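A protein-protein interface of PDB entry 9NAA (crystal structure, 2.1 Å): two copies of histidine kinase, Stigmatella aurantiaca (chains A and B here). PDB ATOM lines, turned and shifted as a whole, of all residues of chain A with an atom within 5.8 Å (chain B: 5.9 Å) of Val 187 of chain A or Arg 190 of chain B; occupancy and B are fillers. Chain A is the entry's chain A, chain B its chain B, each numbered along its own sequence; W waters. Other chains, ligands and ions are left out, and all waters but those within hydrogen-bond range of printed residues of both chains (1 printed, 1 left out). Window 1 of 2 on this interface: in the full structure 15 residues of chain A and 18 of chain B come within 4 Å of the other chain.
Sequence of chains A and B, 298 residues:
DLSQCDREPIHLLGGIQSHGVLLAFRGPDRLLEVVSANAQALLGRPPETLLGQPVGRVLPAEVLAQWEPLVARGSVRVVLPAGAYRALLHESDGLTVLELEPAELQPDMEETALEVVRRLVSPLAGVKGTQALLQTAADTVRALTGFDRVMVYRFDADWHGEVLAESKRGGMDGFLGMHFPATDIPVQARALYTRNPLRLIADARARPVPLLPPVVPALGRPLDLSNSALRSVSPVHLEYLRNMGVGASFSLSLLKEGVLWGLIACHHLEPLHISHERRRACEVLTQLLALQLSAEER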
ATOM      1  N   ASP A   6      -4.441 -16.812 -16.629  1.00  0.00           N
ATOM      2  CA  ASP A   6      -3.987 -15.435 -16.466  1.00  0.00           C
ATOM      3  C   ASP A   6      -3.326 -15.205 -15.115  1.00  0.00           C
ATOM      4  O   ASP A   6      -2.927 -14.072 -14.812  1.00  0.00           O
ATOM      5  CB  ASP A   6      -5.158 -14.459 -16.656  1.00  0.00           C
ATOM      6  CG  ASP A   6      -5.545 -14.263 -18.133  1.00  0.00           C
ATOM      7  OD1 ASP A   6      -4.645 -14.131 -19.005  1.00  0.00           O
ATOM      8  OD2 ASP A   6      -6.762 -14.249 -18.424  1.00  0.00           O
ATOM      9  N   ILE A 185      -3.188 -10.442 -23.005  1.00  0.00           N
ATOM     10  CA  ILE A 185      -1.820 -10.711 -22.581  1.00  0.00           C
ATOM     11  C   ILE A 185      -1.759 -10.492 -21.077  1.00  0.00           C
ATOM     12  O   ILE A 185      -1.947  -9.357 -20.602  1.00  0.00           O
ATOM     13  CB  ILE A 185      -0.812  -9.860 -23.369  1.00  0.00           C
ATOM     14  CG1 ILE A 185      -0.999 -10.117 -24.869  1.00  0.00           C
ATOM     15  CG2 ILE A 185       0.604 -10.194 -22.954  1.00  0.00           C
ATOM     16  CD1 ILE A 185      -0.043  -9.370 -25.727  1.00  0.00           C
ATOM     17  N   PRO A 186      -1.535 -11.552 -20.302  1.00  0.00           N
ATOM     18  CA  PRO A 186      -1.591 -11.441 -18.840  1.00  0.00           C
ATOM     19  C   PRO A 186      -0.488 -10.537 -18.303  1.00  0.00           C
ATOM     20  O   PRO A 186       0.561 -10.344 -18.928  1.00  0.00           O
ATOM     21  CB  PRO A 186      -1.389 -12.887 -18.379  1.00  0.00           C
ATOM     22  CG  PRO A 186      -0.567 -13.498 -19.465  1.00  0.00           C
ATOM     23  CD  PRO A 186      -1.040 -12.869 -20.741  1.00  0.00           C
ATOM     24  N   VAL A 187      -0.717 -10.029 -17.090  1.00  0.00           N
ATOM     25  CA  VAL A 187       0.190  -9.050 -16.502  1.00  0.00           C
ATOM     26  C   VAL A 187       1.608  -9.608 -16.396  1.00  0.00           C
ATOM     27  O   VAL A 187       2.589  -8.891 -16.624  1.00  0.00           O
ATOM     28  CB  VAL A 187      -0.353  -8.562 -15.138  1.00  0.00           C
ATOM     29  CG1 VAL A 187      -0.245  -9.639 -14.053  1.00  0.00           C
ATOM     30  CG2 VAL A 187       0.387  -7.342 -14.718  1.00  0.00           C
ATOM     31  N   GLN A 188       1.746 -10.899 -16.092  1.00  0.00           N
ATOM     32  CA  GLN A 188       3.082 -11.468 -15.947  1.00  0.00           C
ATOM     33  C   GLN A 188       3.836 -11.460 -17.269  1.00  0.00           C
ATOM     34  O   GLN A 188       5.064 -11.313 -17.279  1.00  0.00           O
ATOM     35  CB  GLN A 188       2.986 -12.894 -15.416  1.00  0.00           C
ATOM     36  CG  GLN A 188       2.370 -13.009 -14.023  1.00  0.00           C
ATOM     37  CD  GLN A 188       0.838 -13.084 -14.064  1.00  0.00           C
ATOM     38  OE1 GLN A 188       0.237 -13.329 -15.124  1.00  0.00           O
ATOM     39  NE2 GLN A 188       0.208 -12.952 -12.895  1.00  0.00           N
ATOM     40  N   ALA A 189       3.118 -11.640 -18.387  1.00  0.00           N
ATOM     41  CA  ALA A 189       3.760 -11.574 -19.692  1.00  0.00           C
ATOM     42  C   ALA A 189       4.183 -10.150 -20.015  1.00  0.00           C
ATOM     43  O   ALA A 189       5.315  -9.920 -20.454  1.00  0.00           O
ATOM     44  CB  ALA A 189       2.829 -12.132 -20.772  1.00  0.00           C
ATOM     45  N   ARG A 190       3.308  -9.172 -19.753  1.00  0.00           N
ATOM     46  CA  ARG A 190       3.667  -7.770 -19.968  1.00  0.00           C
ATOM     47  C   ARG A 190       4.803  -7.324 -19.047  1.00  0.00           C
ATOM     48  O   ARG A 190       5.599  -6.455 -19.422  1.00  0.00           O
ATOM     49  CB  ARG A 190       2.429  -6.892 -19.786  1.00  0.00           C
ATOM     50  CG  ARG A 190       1.479  -6.950 -20.995  1.00  0.00           C
ATOM     51  CD  ARG A 190       0.153  -6.184 -20.757  1.00  0.00           C
ATOM     52  NE  ARG A 190      -0.804  -6.910 -19.924  1.00  0.00           N
ATOM     53  CZ  ARG A 190      -1.277  -6.490 -18.756  1.00  0.00           C
ATOM     54  NH1 ARG A 190      -0.885  -5.346 -18.215  1.00  0.00           N
ATOM     55  NH2 ARG A 190      -2.177  -7.234 -18.116  1.00  0.00           N
ATOM     56  N   ALA A 191       4.928  -7.929 -17.859  1.00  0.00           N
ATOM     57  CA  ALA A 191       6.054  -7.579 -16.998  1.00  0.00           C
ATOM     58  C   ALA A 191       7.361  -8.096 -17.578  1.00  0.00           C
ATOM     59  O   ALA A 191       8.401  -7.426 -17.485  1.00  0.00           O
ATOM     60  CB  ALA A 191       5.852  -8.123 -15.581  1.00  0.00           C
ATOM     61  N   LEU A 192       7.333  -9.279 -18.188  1.00  0.00           N
ATOM     62  CA  LEU A 192       8.556  -9.802 -18.790  1.00  0.00           C
ATOM     63  C   LEU A 192       8.926  -9.031 -20.046  1.00  0.00           C
ATOM     64  O   LEU A 192      10.114  -8.836 -20.340  1.00  0.00           O
ATOM     65  CB  LEU A 192       8.390 -11.277 -19.123  1.00  0.00           C
ATOM     66  CG  LEU A 192       8.261 -12.224 -17.947  1.00  0.00           C
ATOM     67  CD1 LEU A 192       8.466 -13.664 -18.487  1.00  0.00           C
ATOM     68  CD2 LEU A 192       9.275 -11.860 -16.867  1.00  0.00           C
ATOM     69  N   LEU B   2      -2.916   2.952 -17.572  1.00  0.00           N
ATOM     70  CA  LEU B   2      -4.213   3.014 -16.891  1.00  0.00           C
ATOM     71  C   LEU B   2      -4.563   4.412 -16.338  1.00  0.00           C
ATOM     72  O   LEU B   2      -5.257   4.499 -15.317  1.00  0.00           O
ATOM     73  CB  LEU B   2      -4.256   1.994 -15.738  1.00  0.00           C
ATOM     74  CG  LEU B   2      -4.043   0.488 -15.921  1.00  0.00           C
ATOM     75  CD1 LEU B   2      -3.651  -0.138 -14.580  1.00  0.00           C
ATOM     76  CD2 LEU B   2      -5.317  -0.165 -16.452  1.00  0.00           C
ATOM     77  N   PHE B 155      -6.595  -9.732  -4.603  1.00  0.00           N
ATOM     78  CA  PHE B 155      -6.831  -9.221  -5.940  1.00  0.00           C
ATOM     79  C   PHE B 155      -7.798 -10.136  -6.676  1.00  0.00           C
ATOM     80  O   PHE B 155      -7.601 -11.354  -6.710  1.00  0.00           O
ATOM     81  CB  PHE B 155      -5.512  -9.108  -6.694  1.00  0.00           C
ATOM     82  CG  PHE B 155      -4.641  -8.014  -6.184  1.00  0.00           C
ATOM     83  CD1 PHE B 155      -5.008  -6.699  -6.360  1.00  0.00           C
ATOM     84  CD2 PHE B 155      -3.476  -8.299  -5.504  1.00  0.00           C
ATOM     85  CE1 PHE B 155      -4.224  -5.692  -5.886  1.00  0.00           C
ATOM     86  CE2 PHE B 155      -2.699  -7.297  -5.015  1.00  0.00           C
ATOM     87  CZ  PHE B 155      -3.059  -5.989  -5.217  1.00  0.00           C
ATOM     88  N   TRP B 159      -7.751  -7.513 -11.179  1.00  0.00           N
ATOM     89  CA  TRP B 159      -6.674  -6.953 -10.363  1.00  0.00           C
ATOM     90  C   TRP B 159      -7.143  -5.759  -9.529  1.00  0.00           C
ATOM     91  O   TRP B 159      -6.365  -4.835  -9.262  1.00  0.00           O
ATOM     92  CB  TRP B 159      -5.467  -6.573 -11.227  1.00  0.00           C
ATOM     93  CG  TRP B 159      -4.767  -7.760 -11.749  1.00  0.00           C
ATOM     94  CD1 TRP B 159      -4.821  -8.240 -13.024  1.00  0.00           C
ATOM     95  CD2 TRP B 159      -3.891  -8.635 -11.026  1.00  0.00           C
ATOM     96  NE1 TRP B 159      -4.050  -9.366 -13.138  1.00  0.00           N
ATOM     97  CE2 TRP B 159      -3.461  -9.630 -11.930  1.00  0.00           C
ATOM     98  CE3 TRP B 159      -3.432  -8.676  -9.706  1.00  0.00           C
ATOM     99  CZ2 TRP B 159      -2.593 -10.657 -11.558  1.00  0.00           C
ATOM    100  CZ3 TRP B 159      -2.574  -9.687  -9.334  1.00  0.00           C
ATOM    101  CH2 TRP B 159      -2.162 -10.671 -10.257  1.00  0.00           C
ATOM    102  N   ILE B 185      -4.440   0.302  -8.503  1.00  0.00           N
ATOM    103  CA  ILE B 185      -3.021   0.021  -8.341  1.00  0.00           C
ATOM    104  C   ILE B 185      -2.450  -0.323  -9.708  1.00  0.00           C
ATOM    105  O   ILE B 185      -2.766  -1.385 -10.258  1.00  0.00           O
ATOM    106  CB  ILE B 185      -2.785  -1.082  -7.299  1.00  0.00           C
ATOM    107  CG1 ILE B 185      -3.429  -0.680  -5.964  1.00  0.00           C
ATOM    108  CG2 ILE B 185      -1.303  -1.310  -7.111  1.00  0.00           C
ATOM    109  CD1 ILE B 185      -3.207  -1.677  -4.826  1.00  0.00           C
ATOM    110  N   PRO B 186      -1.608   0.538 -10.279  1.00  0.00           N
ATOM    111  CA  PRO B 186      -1.121   0.316 -11.648  1.00  0.00           C
ATOM    112  C   PRO B 186      -0.249  -0.926 -11.756  1.00  0.00           C
ATOM    113  O   PRO B 186       0.258  -1.455 -10.766  1.00  0.00           O
ATOM    114  CB  PRO B 186      -0.313   1.582 -11.945  1.00  0.00           C
ATOM    115  CG  PRO B 186       0.149   2.056 -10.578  1.00  0.00           C
ATOM    116  CD  PRO B 186      -0.985   1.715  -9.640  1.00  0.00           C
ATOM    117  N   VAL B 187      -0.090  -1.399 -12.996  1.00  0.00           N
ATOM    118  CA  VAL B 187       0.655  -2.633 -13.228  1.00  0.00           C
ATOM    119  C   VAL B 187       2.082  -2.504 -12.706  1.00  0.00           C
ATOM    120  O   VAL B 187       2.634  -3.451 -12.140  1.00  0.00           O
ATOM    121  CB  VAL B 187       0.624  -3.028 -14.722  1.00  0.00           C
ATOM    122  CG1 VAL B 187      -0.784  -3.255 -15.179  1.00  0.00           C
ATOM    123  CG2 VAL B 187       1.292  -1.975 -15.589  1.00  0.00           C
ATOM    124  N   GLN B 188       2.692  -1.333 -12.851  1.00  0.00           N
ATOM    125  CA  GLN B 188       4.082  -1.192 -12.436  1.00  0.00           C
ATOM    126  C   GLN B 188       4.217  -1.363 -10.927  1.00  0.00           C
ATOM    127  O   GLN B 188       5.202  -1.936 -10.448  1.00  0.00           O
ATOM    128  CB  GLN B 188       4.597   0.180 -12.867  1.00  0.00           C
ATOM    129  CG  GLN B 188       4.600   0.428 -14.365  1.00  0.00           C
ATOM    130  CD  GLN B 188       3.239   0.944 -14.856  1.00  0.00           C
ATOM    131  OE1 GLN B 188       2.420   1.445 -14.068  1.00  0.00           O
ATOM    132  NE2 GLN B 188       3.008   0.845 -16.170  1.00  0.00           N
ATOM    133  N   ALA B 189       3.222  -0.894 -10.168  1.00  0.00           N
ATOM    134  CA  ALA B 189       3.238  -1.096  -8.721  1.00  0.00           C
ATOM    135  C   ALA B 189       3.019  -2.567  -8.367  1.00  0.00           C
ATOM    136  O   ALA B 189       3.705  -3.109  -7.490  1.00  0.00           O
ATOM    137  CB  ALA B 189       2.189  -0.212  -8.045  1.00  0.00           C
ATOM    138  N   ARG B 190       2.074  -3.234  -9.043  1.00  0.00           N
ATOM    139  CA  ARG B 190       1.858  -4.659  -8.781  1.00  0.00           C
ATOM    140  C   ARG B 190       3.052  -5.502  -9.192  1.00  0.00           C
ATOM    141  O   ARG B 190       3.306  -6.543  -8.583  1.00  0.00           O
ATOM    142  CB  ARG B 190       0.584  -5.151  -9.476  1.00  0.00           C
ATOM    143  CG  ARG B 190      -0.677  -4.735  -8.691  1.00  0.00           C
ATOM    144  CD  ARG B 190      -1.972  -5.057  -9.428  1.00  0.00           C
ATOM    145  NE  ARG B 190      -2.264  -4.119 -10.512  1.00  0.00           N
ATOM    146  CZ  ARG B 190      -2.364  -4.440 -11.797  1.00  0.00           C
ATOM    147  NH1 ARG B 190      -2.170  -5.681 -12.224  1.00  0.00           N
ATOM    148  NH2 ARG B 190      -2.687  -3.497 -12.675  1.00  0.00           N
ATOM    149  N   ALA B 191       3.814  -5.064 -10.188  1.00  0.00           N
ATOM    150  CA  ALA B 191       4.983  -5.834 -10.590  1.00  0.00           C
ATOM    151  C   ALA B 191       6.058  -5.778  -9.515  1.00  0.00           C
ATOM    152  O   ALA B 191       6.775  -6.764  -9.281  1.00  0.00           O
ATOM    153  CB  ALA B 191       5.530  -5.311 -11.918  1.00  0.00           C
ATOM    154  N   LEU B 192       6.192  -4.622  -8.864  1.00  0.00           N
ATOM    155  CA  LEU B 192       7.164  -4.487  -7.789  1.00  0.00           C
ATOM    156  C   LEU B 192       6.704  -5.214  -6.537  1.00  0.00           C
ATOM    157  O   LEU B 192       7.540  -5.720  -5.782  1.00  0.00           O
ATOM    158  CB  LEU B 192       7.422  -3.008  -7.479  1.00  0.00           C
ATOM    159  CG  LEU B 192       8.122  -2.241  -8.600  1.00  0.00           C
ATOM    160  CD1 LEU B 192       8.657  -0.899  -8.059  1.00  0.00           C
ATOM    161  CD2 LEU B 192       9.237  -3.044  -9.232  1.00  0.00           C
ATOM    162  N   TYR B 193       5.392  -5.245  -6.283  1.00  0.00           N
ATOM    163  CA  TYR B 193       4.897  -6.029  -5.154  1.00  0.00           C
ATOM    164  C   TYR B 193       5.173  -7.510  -5.360  1.00  0.00           C
ATOM    165  O   TYR B 193       5.375  -8.251  -4.388  1.00  0.00           O
ATOM    166  CB  TYR B 193       3.399  -5.803  -4.947  1.00  0.00           C
ATOM    167  CG  TYR B 193       2.967  -4.473  -4.357  1.00  0.00           C
ATOM    168  CD1 TYR B 193       3.603  -3.944  -3.240  1.00  0.00           C
ATOM    169  CD2 TYR B 193       1.856  -3.798  -4.855  1.00  0.00           C
ATOM    170  CE1 TYR B 193       3.182  -2.740  -2.664  1.00  0.00           C
ATOM    171  CE2 TYR B 193       1.426  -2.605  -4.294  1.00  0.00           C
ATOM    172  CZ  TYR B 193       2.089  -2.079  -3.191  1.00  0.00           C
ATOM    173  OH  TYR B 193       1.669  -0.892  -2.622  1.00  0.00           O
ATOM    174  N   THR B 194       5.176  -7.953  -6.624  1.00  0.00           N
ATOM    175  CA  THR B 194       5.486  -9.340  -6.945  1.00  0.00           C
ATOM    176  C   THR B 194       6.965  -9.617  -6.741  1.00  0.00           C
ATOM    177  O   THR B 194       7.342 -10.666  -6.210  1.00  0.00           O
ATOM    178  CB  THR B 194       5.083  -9.646  -8.395  1.00  0.00           C
ATOM    179  OG1 THR B 194       3.700  -9.311  -8.584  1.00  0.00           O
ATOM    180  CG2 THR B 194       5.279 -11.132  -8.715  1.00  0.00           C
ATOM    181  N   ARG B 195       7.820  -8.679  -7.125  1.00  0.00           N
ATOM    182  CA  ARG B 195       9.252  -8.934  -7.018  1.00  0.00           C
ATOM    183  C   ARG B 195       9.818  -8.684  -5.615  1.00  0.00           C
ATOM    184  O   ARG B 195      10.873  -9.229  -5.282  1.00  0.00           O
ATOM    185  CB  ARG B 195      10.017  -8.086  -8.046  1.00  0.00           C
ATOM    186  CG  ARG B 195       9.694  -8.364  -9.509  1.00  0.00           C
ATOM    187  CD  ARG B 195      10.303  -7.295 -10.423  1.00  0.00           C
ATOM    188  NE  ARG B 195      11.764  -7.307 -10.439  1.00  0.00           N
ATOM    189  CZ  ARG B 195      12.522  -6.494 -11.171  1.00  0.00           C
ATOM    190  NH1 ARG B 195      11.995  -5.551 -11.940  1.00  0.00           N
ATOM    191  NH2 ARG B 195      13.846  -6.637 -11.142  1.00  0.00           N
ATOM    192  N   LEU B 260       1.305 -12.898  -7.800  1.00  0.00           N
ATOM    193  CA  LEU B 260       0.760 -11.979  -6.806  1.00  0.00           C
ATOM    194  C   LEU B 260      -0.706 -12.293  -6.563  1.00  0.00           C
ATOM    195  O   LEU B 260      -1.507 -12.349  -7.499  1.00  0.00           O
ATOM    196  CB  LEU B 260       0.912 -10.528  -7.268  1.00  0.00           C
ATOM    197  CG  LEU B 260       0.440  -9.468  -6.264  1.00  0.00           C
ATOM    198  CD1 LEU B 260       1.334  -9.506  -5.054  1.00  0.00           C
ATOM    199  CD2 LEU B 260       0.364  -8.042  -6.870  1.00  0.00           C
HETATM  200  O   HOH W   1      -3.314 -10.943 -15.797  1.00  0.00           O
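O of Asp 6 of chain A lies close to OE1 of Gln 188 of chain A (3.3 Å).
O of Ile 185 of chain B lies within hydrogen-bond range of NE of Arg 190 of chain B (2.8 Å).
The guanidinium group (NE) of Arg 190 of chain A sits at hydrogen-bond distance from the backbone carbonyl oxygen (O) of Ile 185 of chain A (2.8 Å).
The backbone carbonyl oxygen (O) of Arg 190 of chain B lies within hydrogen-bond range of the side-chain hydroxyl (OG1) of Thr 194 of chain B.
CG1 of Val 187 of chain A touches CZ2 of Trp 159 of chain B, 3.6 Å away.
Val 187 of chain A touches Arg 190 of chain B (CG2 to NH1, 3.9 Å).
Trp 159 of chain B touches Gln 188 of chain A (CZ2 to NE2, 3.9 Å).
Val 187 of chain B touches Arg 190 of chain A.
Val 187 of chain A touches just these residues of chain B: Trp 159 and Arg 190.
Of the printed residues of chain B, Arg 190 of chain A touches Val 187.
Printed residues of chain A within 4 Å of Val 187 of chain B: Arg 190 (3.7 Å).
Printed residues of chain A within 4 Å of Trp 159 of chain B: Val 187 (3.6 Å) and Gln 188 (3.9 Å).
Ala 189 of chain B touches none of the printed residues of chain A.
Leu 192 of chain B touches none of the printed residues of chain A.
The nearest residue of chain B that does not touch Val 187 of chain A is Val 187 of chain B (4.3 Å).
Printed residues of chain B that touch a printed residue of chain A: Trp 159, Val 187 and Arg 190.
Hydrophobic or aromatic side chains of chain B within 4 Å of the printed part of chain A: Trp 159 and Val 187.
Along chain B the printed residues that touch a printed residue of chain A span positions 159 to 190.
Hydrophobic or aromatic side chains of chain A within 4 Å of the printed part of chain B: Val 187.
Among the printed residues, no Asp or Glu carboxylate lies within 4 Å of a Lys or Arg side-chain nitrogen of the other chain.
Val 187 of chain A touches Arg 190 of chain B, and with the chains exchanged Arg 190 of chain A touches Val 187 of chain B.
Of the 4 pairs that touch across the chains among the printed residues, 2 have their exchanged pair printed and touching as well.
Water W1 lies within hydrogen-bond range of N of Val 187 of chain A (3.0 Å), NE1 of Trp 159 of chain B (3.2 Å) and O of Asp 6 of chain A (3.3 Å).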
